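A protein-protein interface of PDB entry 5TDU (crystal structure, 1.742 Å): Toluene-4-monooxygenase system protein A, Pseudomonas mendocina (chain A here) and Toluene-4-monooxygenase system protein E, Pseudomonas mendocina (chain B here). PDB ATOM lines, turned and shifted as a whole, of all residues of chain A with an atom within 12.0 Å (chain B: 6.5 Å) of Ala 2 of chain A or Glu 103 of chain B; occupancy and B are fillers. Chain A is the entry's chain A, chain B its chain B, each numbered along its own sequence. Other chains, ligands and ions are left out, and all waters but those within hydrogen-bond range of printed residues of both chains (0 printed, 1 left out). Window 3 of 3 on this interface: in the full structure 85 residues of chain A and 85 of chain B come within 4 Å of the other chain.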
ATOM      1  N   ALA A   2       7.462 -25.276  -8.099  1.00  0.00           N
ATOM      2  CA  ALA A   2       7.678 -24.261  -9.120  1.00  0.00           C
ATOM      3  C   ALA A   2       8.159 -22.964  -8.486  1.00  0.00           C
ATOM      4  O   ALA A   2       7.957 -22.740  -7.290  1.00  0.00           O
ATOM      5  CB  ALA A   2       6.401 -24.020  -9.916  1.00  0.00           C
ATOM      6  N   MET A   3       8.803 -22.124  -9.299  1.00  0.00           N
ATOM      7  CA  MET A   3       9.255 -20.792  -8.893  1.00  0.00           C
ATOM      8  C   MET A   3       8.477 -19.737  -9.667  1.00  0.00           C
ATOM      9  O   MET A   3       8.037 -19.972 -10.796  1.00  0.00           O
ATOM     10  CB  MET A   3      10.756 -20.604  -9.144  1.00  0.00           C
ATOM     11  CG  MET A   3      11.640 -21.640  -8.467  1.00  0.00           C
ATOM     12  SD  MET A   3      11.487 -21.546  -6.673  1.00  0.00           S
ATOM     13  CE  MET A   3      12.166 -19.911  -6.348  1.00  0.00           C
ATOM     14  N   HIS A   4       8.313 -18.568  -9.061  1.00  0.00           N
ATOM     15  CA  HIS A   4       7.595 -17.489  -9.713  1.00  0.00           C
ATOM     16  C   HIS A   4       8.591 -16.486 -10.271  1.00  0.00           C
ATOM     17  O   HIS A   4       9.576 -16.171  -9.618  1.00  0.00           O
ATOM     18  CB  HIS A   4       6.625 -16.855  -8.717  1.00  0.00           C
ATOM     19  CG  HIS A   4       5.835 -17.873  -7.962  1.00  0.00           C
ATOM     20  ND1 HIS A   4       4.882 -18.666  -8.568  1.00  0.00           N
ATOM     21  CD2 HIS A   4       5.900 -18.280  -6.673  1.00  0.00           C
ATOM     22  CE1 HIS A   4       4.375 -19.496  -7.676  1.00  0.00           C
ATOM     23  NE2 HIS A   4       4.979 -19.286  -6.519  1.00  0.00           N
ATOM     24  N   PRO A   5       8.346 -16.011 -11.503  1.00  0.00           N
ATOM     25  CA  PRO A   5       9.300 -15.146 -12.201  1.00  0.00           C
ATOM     26  C   PRO A   5       9.441 -13.791 -11.513  1.00  0.00           C
ATOM     27  O   PRO A   5       8.475 -13.290 -10.923  1.00  0.00           O
ATOM     28  CB  PRO A   5       8.693 -15.003 -13.607  1.00  0.00           C
ATOM     29  CG  PRO A   5       7.253 -15.315 -13.444  1.00  0.00           C
ATOM     30  CD  PRO A   5       7.171 -16.332 -12.336  1.00  0.00           C
ATOM     31  N   ARG A   6      10.638 -13.213 -11.581  1.00  0.00           N
ATOM     32  CA  ARG A   6      10.928 -11.949 -10.901  1.00  0.00           C
ATOM     33  C   ARG A   6       9.904 -10.849 -11.196  1.00  0.00           C
ATOM     34  O   ARG A   6       9.555 -10.059 -10.309  1.00  0.00           O
ATOM     35  CB  ARG A   6      12.323 -11.459 -11.283  1.00  0.00           C
ATOM     36  CG  ARG A   6      12.799 -10.262 -10.465  1.00  0.00           C
ATOM     37  CD  ARG A   6      14.200  -9.873 -10.852  1.00  0.00           C
ATOM     38  NE  ARG A   6      14.227  -9.204 -12.153  1.00  0.00           N
ATOM     39  CZ  ARG A   6      15.319  -9.045 -12.893  1.00  0.00           C
ATOM     40  NH1 ARG A   6      16.484  -9.527 -12.477  1.00  0.00           N
ATOM     41  NH2 ARG A   6      15.239  -8.419 -14.063  1.00  0.00           N
ATOM     42  N   ASP A   8       6.883 -10.864 -11.385  1.00  0.00           N
ATOM     43  CA  ASP A   8       5.655 -10.995 -10.602  1.00  0.00           C
ATOM     44  C   ASP A   8       5.796 -10.568  -9.137  1.00  0.00           C
ATOM     45  O   ASP A   8       4.797 -10.294  -8.486  1.00  0.00           O
ATOM     46  CB  ASP A   8       5.138 -12.435 -10.648  1.00  0.00           C
ATOM     47  CG  ASP A   8       4.660 -12.847 -12.026  1.00  0.00           C
ATOM     48  OD1 ASP A   8       4.564 -11.987 -12.921  1.00  0.00           O
ATOM     49  OD2 ASP A   8       4.358 -14.038 -12.205  1.00  0.00           O
ATOM     50  N   TRP A   9       7.017 -10.509  -8.610  1.00  0.00           N
ATOM     51  CA  TRP A   9       7.188 -10.113  -7.211  1.00  0.00           C
ATOM     52  C   TRP A   9       8.160  -8.943  -7.050  1.00  0.00           C
ATOM     53  O   TRP A   9       8.350  -8.463  -5.935  1.00  0.00           O
ATOM     54  CB  TRP A   9       7.652 -11.312  -6.351  1.00  0.00           C
ATOM     55  CG  TRP A   9       8.797 -12.127  -6.939  1.00  0.00           C
ATOM     56  CD1 TRP A   9       8.687 -13.280  -7.673  1.00  0.00           C
ATOM     57  CD2 TRP A   9      10.203 -11.854  -6.836  1.00  0.00           C
ATOM     58  NE1 TRP A   9       9.934 -13.735  -8.035  1.00  0.00           N
ATOM     59  CE2 TRP A   9      10.881 -12.880  -7.533  1.00  0.00           C
ATOM     60  CE3 TRP A   9      10.953 -10.838  -6.232  1.00  0.00           C
ATOM     61  CZ2 TRP A   9      12.277 -12.923  -7.638  1.00  0.00           C
ATOM     62  CZ3 TRP A   9      12.347 -10.883  -6.334  1.00  0.00           C
ATOM     63  CH2 TRP A   9      12.991 -11.917  -7.033  1.00  0.00           C
ATOM     64  N   PHE B  98      11.615 -23.164  -1.333  1.00  0.00           N
ATOM     65  CA  PHE B  98      10.467 -22.504  -1.973  1.00  0.00           C
ATOM     66  C   PHE B  98       9.924 -23.373  -3.110  1.00  0.00           C
ATOM     67  O   PHE B  98       8.722 -23.599  -3.224  1.00  0.00           O
ATOM     68  CB  PHE B  98      10.848 -21.126  -2.530  1.00  0.00           C
ATOM     69  CG  PHE B  98      11.089 -20.069  -1.481  1.00  0.00           C
ATOM     70  CD1 PHE B  98      11.635 -18.844  -1.851  1.00  0.00           C
ATOM     71  CD2 PHE B  98      10.764 -20.282  -0.143  1.00  0.00           C
ATOM     72  CE1 PHE B  98      11.859 -17.836  -0.904  1.00  0.00           C
ATOM     73  CE2 PHE B  98      10.990 -19.289   0.810  1.00  0.00           C
ATOM     74  CZ  PHE B  98      11.534 -18.061   0.427  1.00  0.00           C
ATOM     75  N   ASP B  99      10.822 -23.855  -3.961  1.00  0.00           N
ATOM     76  CA  ASP B  99      10.419 -24.651  -5.112  1.00  0.00           C
ATOM     77  C   ASP B  99       9.682 -25.910  -4.654  1.00  0.00           C
ATOM     78  O   ASP B  99       8.557 -26.185  -5.091  1.00  0.00           O
ATOM     79  CB  ASP B  99      11.646 -25.015  -5.953  1.00  0.00           C
ATOM     80  CG  ASP B  99      11.288 -25.654  -7.275  1.00  0.00           C
ATOM     81  OD1 ASP B  99      10.137 -25.509  -7.729  1.00  0.00           O
ATOM     82  OD2 ASP B  99      12.180 -26.293  -7.876  1.00  0.00           O
ATOM     83  N   GLN B 100      10.312 -26.663  -3.758  1.00  0.00           N
ATOM     84  CA  GLN B 100       9.769 -27.945  -3.325  1.00  0.00           C
ATOM     85  C   GLN B 100       8.478 -27.794  -2.526  1.00  0.00           C
ATOM     86  O   GLN B 100       7.541 -28.571  -2.710  1.00  0.00           O
ATOM     87  CB  GLN B 100      10.806 -28.715  -2.501  1.00  0.00           C
ATOM     88  CG  GLN B 100      10.318 -30.091  -2.059  1.00  0.00           C
ATOM     89  CD  GLN B 100       9.817 -30.931  -3.223  1.00  0.00           C
ATOM     90  OE1 GLN B 100       8.780 -31.591  -3.130  1.00  0.00           O
ATOM     91  NE2 GLN B 100      10.544 -30.898  -4.331  1.00  0.00           N
ATOM     92  N   PHE B 101       8.409 -26.797  -1.646  1.00  0.00           N
ATOM     93  CA  PHE B 101       7.194 -26.627  -0.860  1.00  0.00           C
ATOM     94  C   PHE B 101       6.052 -26.143  -1.752  1.00  0.00           C
ATOM     95  O   PHE B 101       4.893 -26.476  -1.523  1.00  0.00           O
ATOM     96  CB  PHE B 101       7.437 -25.678   0.321  1.00  0.00           C
ATOM     97  CG  PHE B 101       8.017 -26.365   1.526  1.00  0.00           C
ATOM     98  CD1 PHE B 101       7.250 -26.569   2.668  1.00  0.00           C
ATOM     99  CD2 PHE B 101       9.314 -26.847   1.502  1.00  0.00           C
ATOM    100  CE1 PHE B 101       7.782 -27.223   3.778  1.00  0.00           C
ATOM    101  CE2 PHE B 101       9.852 -27.503   2.603  1.00  0.00           C
ATOM    102  CZ  PHE B 101       9.089 -27.690   3.741  1.00  0.00           C
ATOM    103  N   ASN B 102       6.379 -25.384  -2.791  1.00  0.00           N
ATOM    104  CA  ASN B 102       5.369 -24.986  -3.763  1.00  0.00           C
ATOM    105  C   ASN B 102       4.870 -26.198  -4.574  1.00  0.00           C
ATOM    106  O   ASN B 102       3.678 -26.308  -4.858  1.00  0.00           O
ATOM    107  CB  ASN B 102       5.922 -23.903  -4.694  1.00  0.00           C
ATOM    108  CG  ASN B 102       5.044 -23.681  -5.899  1.00  0.00           C
ATOM    109  OD1 ASN B 102       5.112 -24.428  -6.877  1.00  0.00           O
ATOM    110  ND2 ASN B 102       4.205 -22.653  -5.837  1.00  0.00           N
ATOM    111  N   GLU B 103       5.775 -27.101  -4.952  1.00  0.00           N
ATOM    112  CA  GLU B 103       5.373 -28.324  -5.652  1.00  0.00           C
ATOM    113  C   GLU B 103       4.375 -29.129  -4.831  1.00  0.00           C
ATOM    114  O   GLU B 103       3.430 -29.724  -5.374  1.00  0.00           O
ATOM    115  CB  GLU B 103       6.591 -29.200  -5.966  1.00  0.00           C
ATOM    116  CG  GLU B 103       7.457 -28.687  -7.089  1.00  0.00           C
ATOM    117  CD  GLU B 103       6.745 -28.723  -8.427  1.00  0.00           C
ATOM    118  OE1 GLU B 103       6.642 -27.655  -9.070  1.00  0.00           O
ATOM    119  OE2 GLU B 103       6.288 -29.821  -8.830  1.00  0.00           O
ATOM    120  N   ARG B 104       4.596 -29.154  -3.520  1.00  0.00           N
ATOM    121  CA  ARG B 104       3.770 -29.924  -2.594  1.00  0.00           C
ATOM    122  C   ARG B 104       2.510 -29.175  -2.165  1.00  0.00           C
ATOM    123  O   ARG B 104       1.714 -29.690  -1.376  1.00  0.00           O
ATOM    124  CB  ARG B 104       4.588 -30.316  -1.356  1.00  0.00           C
ATOM    125  CG  ARG B 104       5.163 -31.726  -1.410  1.00  0.00           C
ATOM    126  CD  ARG B 104       6.653 -31.767  -1.088  1.00  0.00           C
ATOM    127  NE  ARG B 104       6.955 -31.516   0.320  1.00  0.00           N
ATOM    128  CZ  ARG B 104       6.991 -32.455   1.262  1.00  0.00           C
ATOM    129  NH1 ARG B 104       7.283 -32.126   2.513  1.00  0.00           N
ATOM    130  NH2 ARG B 104       6.731 -33.721   0.959  1.00  0.00           N
ATOM    131  N   GLU B 105       2.332 -27.957  -2.670  1.00  0.00           N
ATOM    132  CA  GLU B 105       1.145 -27.166  -2.338  1.00  0.00           C
ATOM    133  C   GLU B 105       1.043 -26.902  -0.835  1.00  0.00           C
ATOM    134  O   GLU B 105      -0.046 -26.931  -0.256  1.00  0.00           O
ATOM    135  CB  GLU B 105      -0.128 -27.865  -2.826  1.00  0.00           C
ATOM    136  CG  GLU B 105      -0.271 -27.937  -4.336  1.00  0.00           C
ATOM    137  CD  GLU B 105      -1.499 -28.729  -4.760  1.00  0.00           C
ATOM    138  OE1 GLU B 105      -1.470 -29.977  -4.666  1.00  0.00           O
ATOM    139  OE2 GLU B 105      -2.501 -28.106  -5.176  1.00  0.00           O
ATOM    140  N   HIS B 106       2.191 -26.643  -0.216  1.00  0.00           N
ATOM    141  CA  HIS B 106       2.271 -26.340   1.208  1.00  0.00           C
ATOM    142  C   HIS B 106       1.225 -25.321   1.668  1.00  0.00           C
ATOM    143  O   HIS B 106       0.550 -25.518   2.681  1.00  0.00           O
ATOM    144  CB  HIS B 106       3.675 -25.824   1.550  1.00  0.00           C
ATOM    145  CG  HIS B 106       3.768 -25.164   2.891  1.00  0.00           C
ATOM    146  ND1 HIS B 106       3.525 -23.817   3.079  1.00  0.00           N
ATOM    147  CD2 HIS B 106       4.069 -25.667   4.112  1.00  0.00           C
ATOM    148  CE1 HIS B 106       3.676 -23.523   4.359  1.00  0.00           C
ATOM    149  NE2 HIS B 106       4.005 -24.627   5.007  1.00  0.00           N
ATOM    150  N   TYR B 168       8.887 -12.170  -1.897  1.00  0.00           N
ATOM    151  CA  TYR B 168       8.611 -13.375  -2.670  1.00  0.00           C
ATOM    152  C   TYR B 168       7.456 -14.172  -2.054  1.00  0.00           C
ATOM    153  O   TYR B 168       6.520 -14.577  -2.752  1.00  0.00           O
ATOM    154  CB  TYR B 168       9.866 -14.252  -2.764  1.00  0.00           C
ATOM    155  CG  TYR B 168       9.663 -15.455  -3.668  1.00  0.00           C
ATOM    156  CD1 TYR B 168       9.963 -15.383  -5.021  1.00  0.00           C
ATOM    157  CD2 TYR B 168       9.142 -16.653  -3.169  1.00  0.00           C
ATOM    158  CE1 TYR B 168       9.767 -16.474  -5.858  1.00  0.00           C
ATOM    159  CE2 TYR B 168       8.943 -17.754  -4.000  1.00  0.00           C
ATOM    160  CZ  TYR B 168       9.250 -17.655  -5.339  1.00  0.00           C
ATOM    161  OH  TYR B 168       9.047 -18.735  -6.167  1.00  0.00           O
ATOM    162  N   GLU B 172       3.736 -15.097  -3.356  1.00  0.00           N
ATOM    163  CA  GLU B 172       3.384 -16.506  -3.540  1.00  0.00           C
ATOM    164  C   GLU B 172       2.138 -16.874  -2.735  1.00  0.00           C
ATOM    165  O   GLU B 172       1.231 -17.568  -3.231  1.00  0.00           O
ATOM    166  CB  GLU B 172       4.548 -17.414  -3.144  1.00  0.00           C
ATOM    167  CG  GLU B 172       4.230 -18.887  -3.336  1.00  0.00           C
ATOM    168  CD  GLU B 172       5.465 -19.754  -3.268  1.00  0.00           C
ATOM    169  OE1 GLU B 172       5.681 -20.560  -4.197  1.00  0.00           O
ATOM    170  OE2 GLU B 172       6.223 -19.631  -2.287  1.00  0.00           O
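The side-chain carboxylate (OD1) of Asp 99 of chain B lies within hydrogen-bond range of the backbone NH (N) of Ala 2 of chain A, 2.7 Å away. The backbone NH of Ala 2 of chain A sits at hydrogen-bond distance from the side-chain amide oxygen of Asn 102 of chain B (2.8 Å). The backbone NH of Ala 2 of chain A sits at hydrogen-bond distance from the side-chain carboxylate of Glu 103 of chain B (2.7 Å). The side-chain sulfur (SD) of Met 3 of chain A lies close to the backbone NH (N) of Asp 99 of chain B (3.6 Å). The side-chain sulfur of Met 3 of chain A sits close to the side-chain hydroxyl of Tyr 168 of chain B (3.8 Å). The side-chain hydroxyl (OH) of Tyr 168 of chain B lies within hydrogen-bond range of the backbone NH (N) of His 4 of chain A (3.0 Å). A ring nitrogen (NE2) of His 4 of chain A lies within hydrogen-bond range of the side-chain carboxylate (OE1) of Glu 172 of chain B, 2.7 Å away.
The backbone carbonyl oxygen of His 4 of chain A lies within hydrogen-bond range of the indole nitrogen of Trp 9 of chain A (2.9 Å). The backbone carbonyl oxygen (O) of Pro 5 of chain A sits close to the indole nitrogen (NE1) of Trp 9 of chain A (3.3 Å). The side-chain amide nitrogen (ND2) of Asn 102 of chain B sits at hydrogen-bond distance from the side-chain carboxylate (OE1) of Glu 172 of chain B, 3.0 Å away.
Among the printed residues, merely in contact across the chains: His 4 of chain A with Asn 102 of chain B (3.5 Å) and Trp 9 of chain A with Tyr 168 of chain B (3.4 Å).
Of chain B, only Asp 99 (2.7 Å), Asn 102 (2.8 Å) and Glu 103 (2.7 Å) come within 4 Å of Ala 2 of chain A. Of the printed residues of chain B, His 4 of chain A touches Asn 102, Tyr 168 and Glu 172. Of the printed residues of chain B, Trp 9 of chain A touches Tyr 168. Asp 99 of chain B touches just these residues of chain A: Ala 2 and Met 3. Asn 102 of chain B touches just these residues of chain A: Ala 2 and His 4. Of chain A, only Ala 2 (2.7 Å) comes within 4 Å of Glu 103 of chain B. Glu 105 of chain B touches none of the printed residues of chain A. Of the printed residues of chain A, Tyr 168 of chain B touches Met 3, His 4 and Trp 9. The nearest residue of chain A that does not touch Glu 103 of chain B is Met 3 of chain A (5.9 Å).
Hydrophobic or aromatic side chains of chain B that line the printed part of chain A: Tyr 168. Of the 7 printed residues of chain A, 4 touch a printed residue of chain B. Hydrophobic or aromatic side chains of chain A that line the printed part of chain B: Ala 2, Met 3, His 4 and Trp 9. Among the printed residues, 9 pairs touch across the chains. Among the printed residues, no Asp or Glu carboxylate lies within 4 Å of a Lys or Arg side-chain nitrogen of the other chain.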
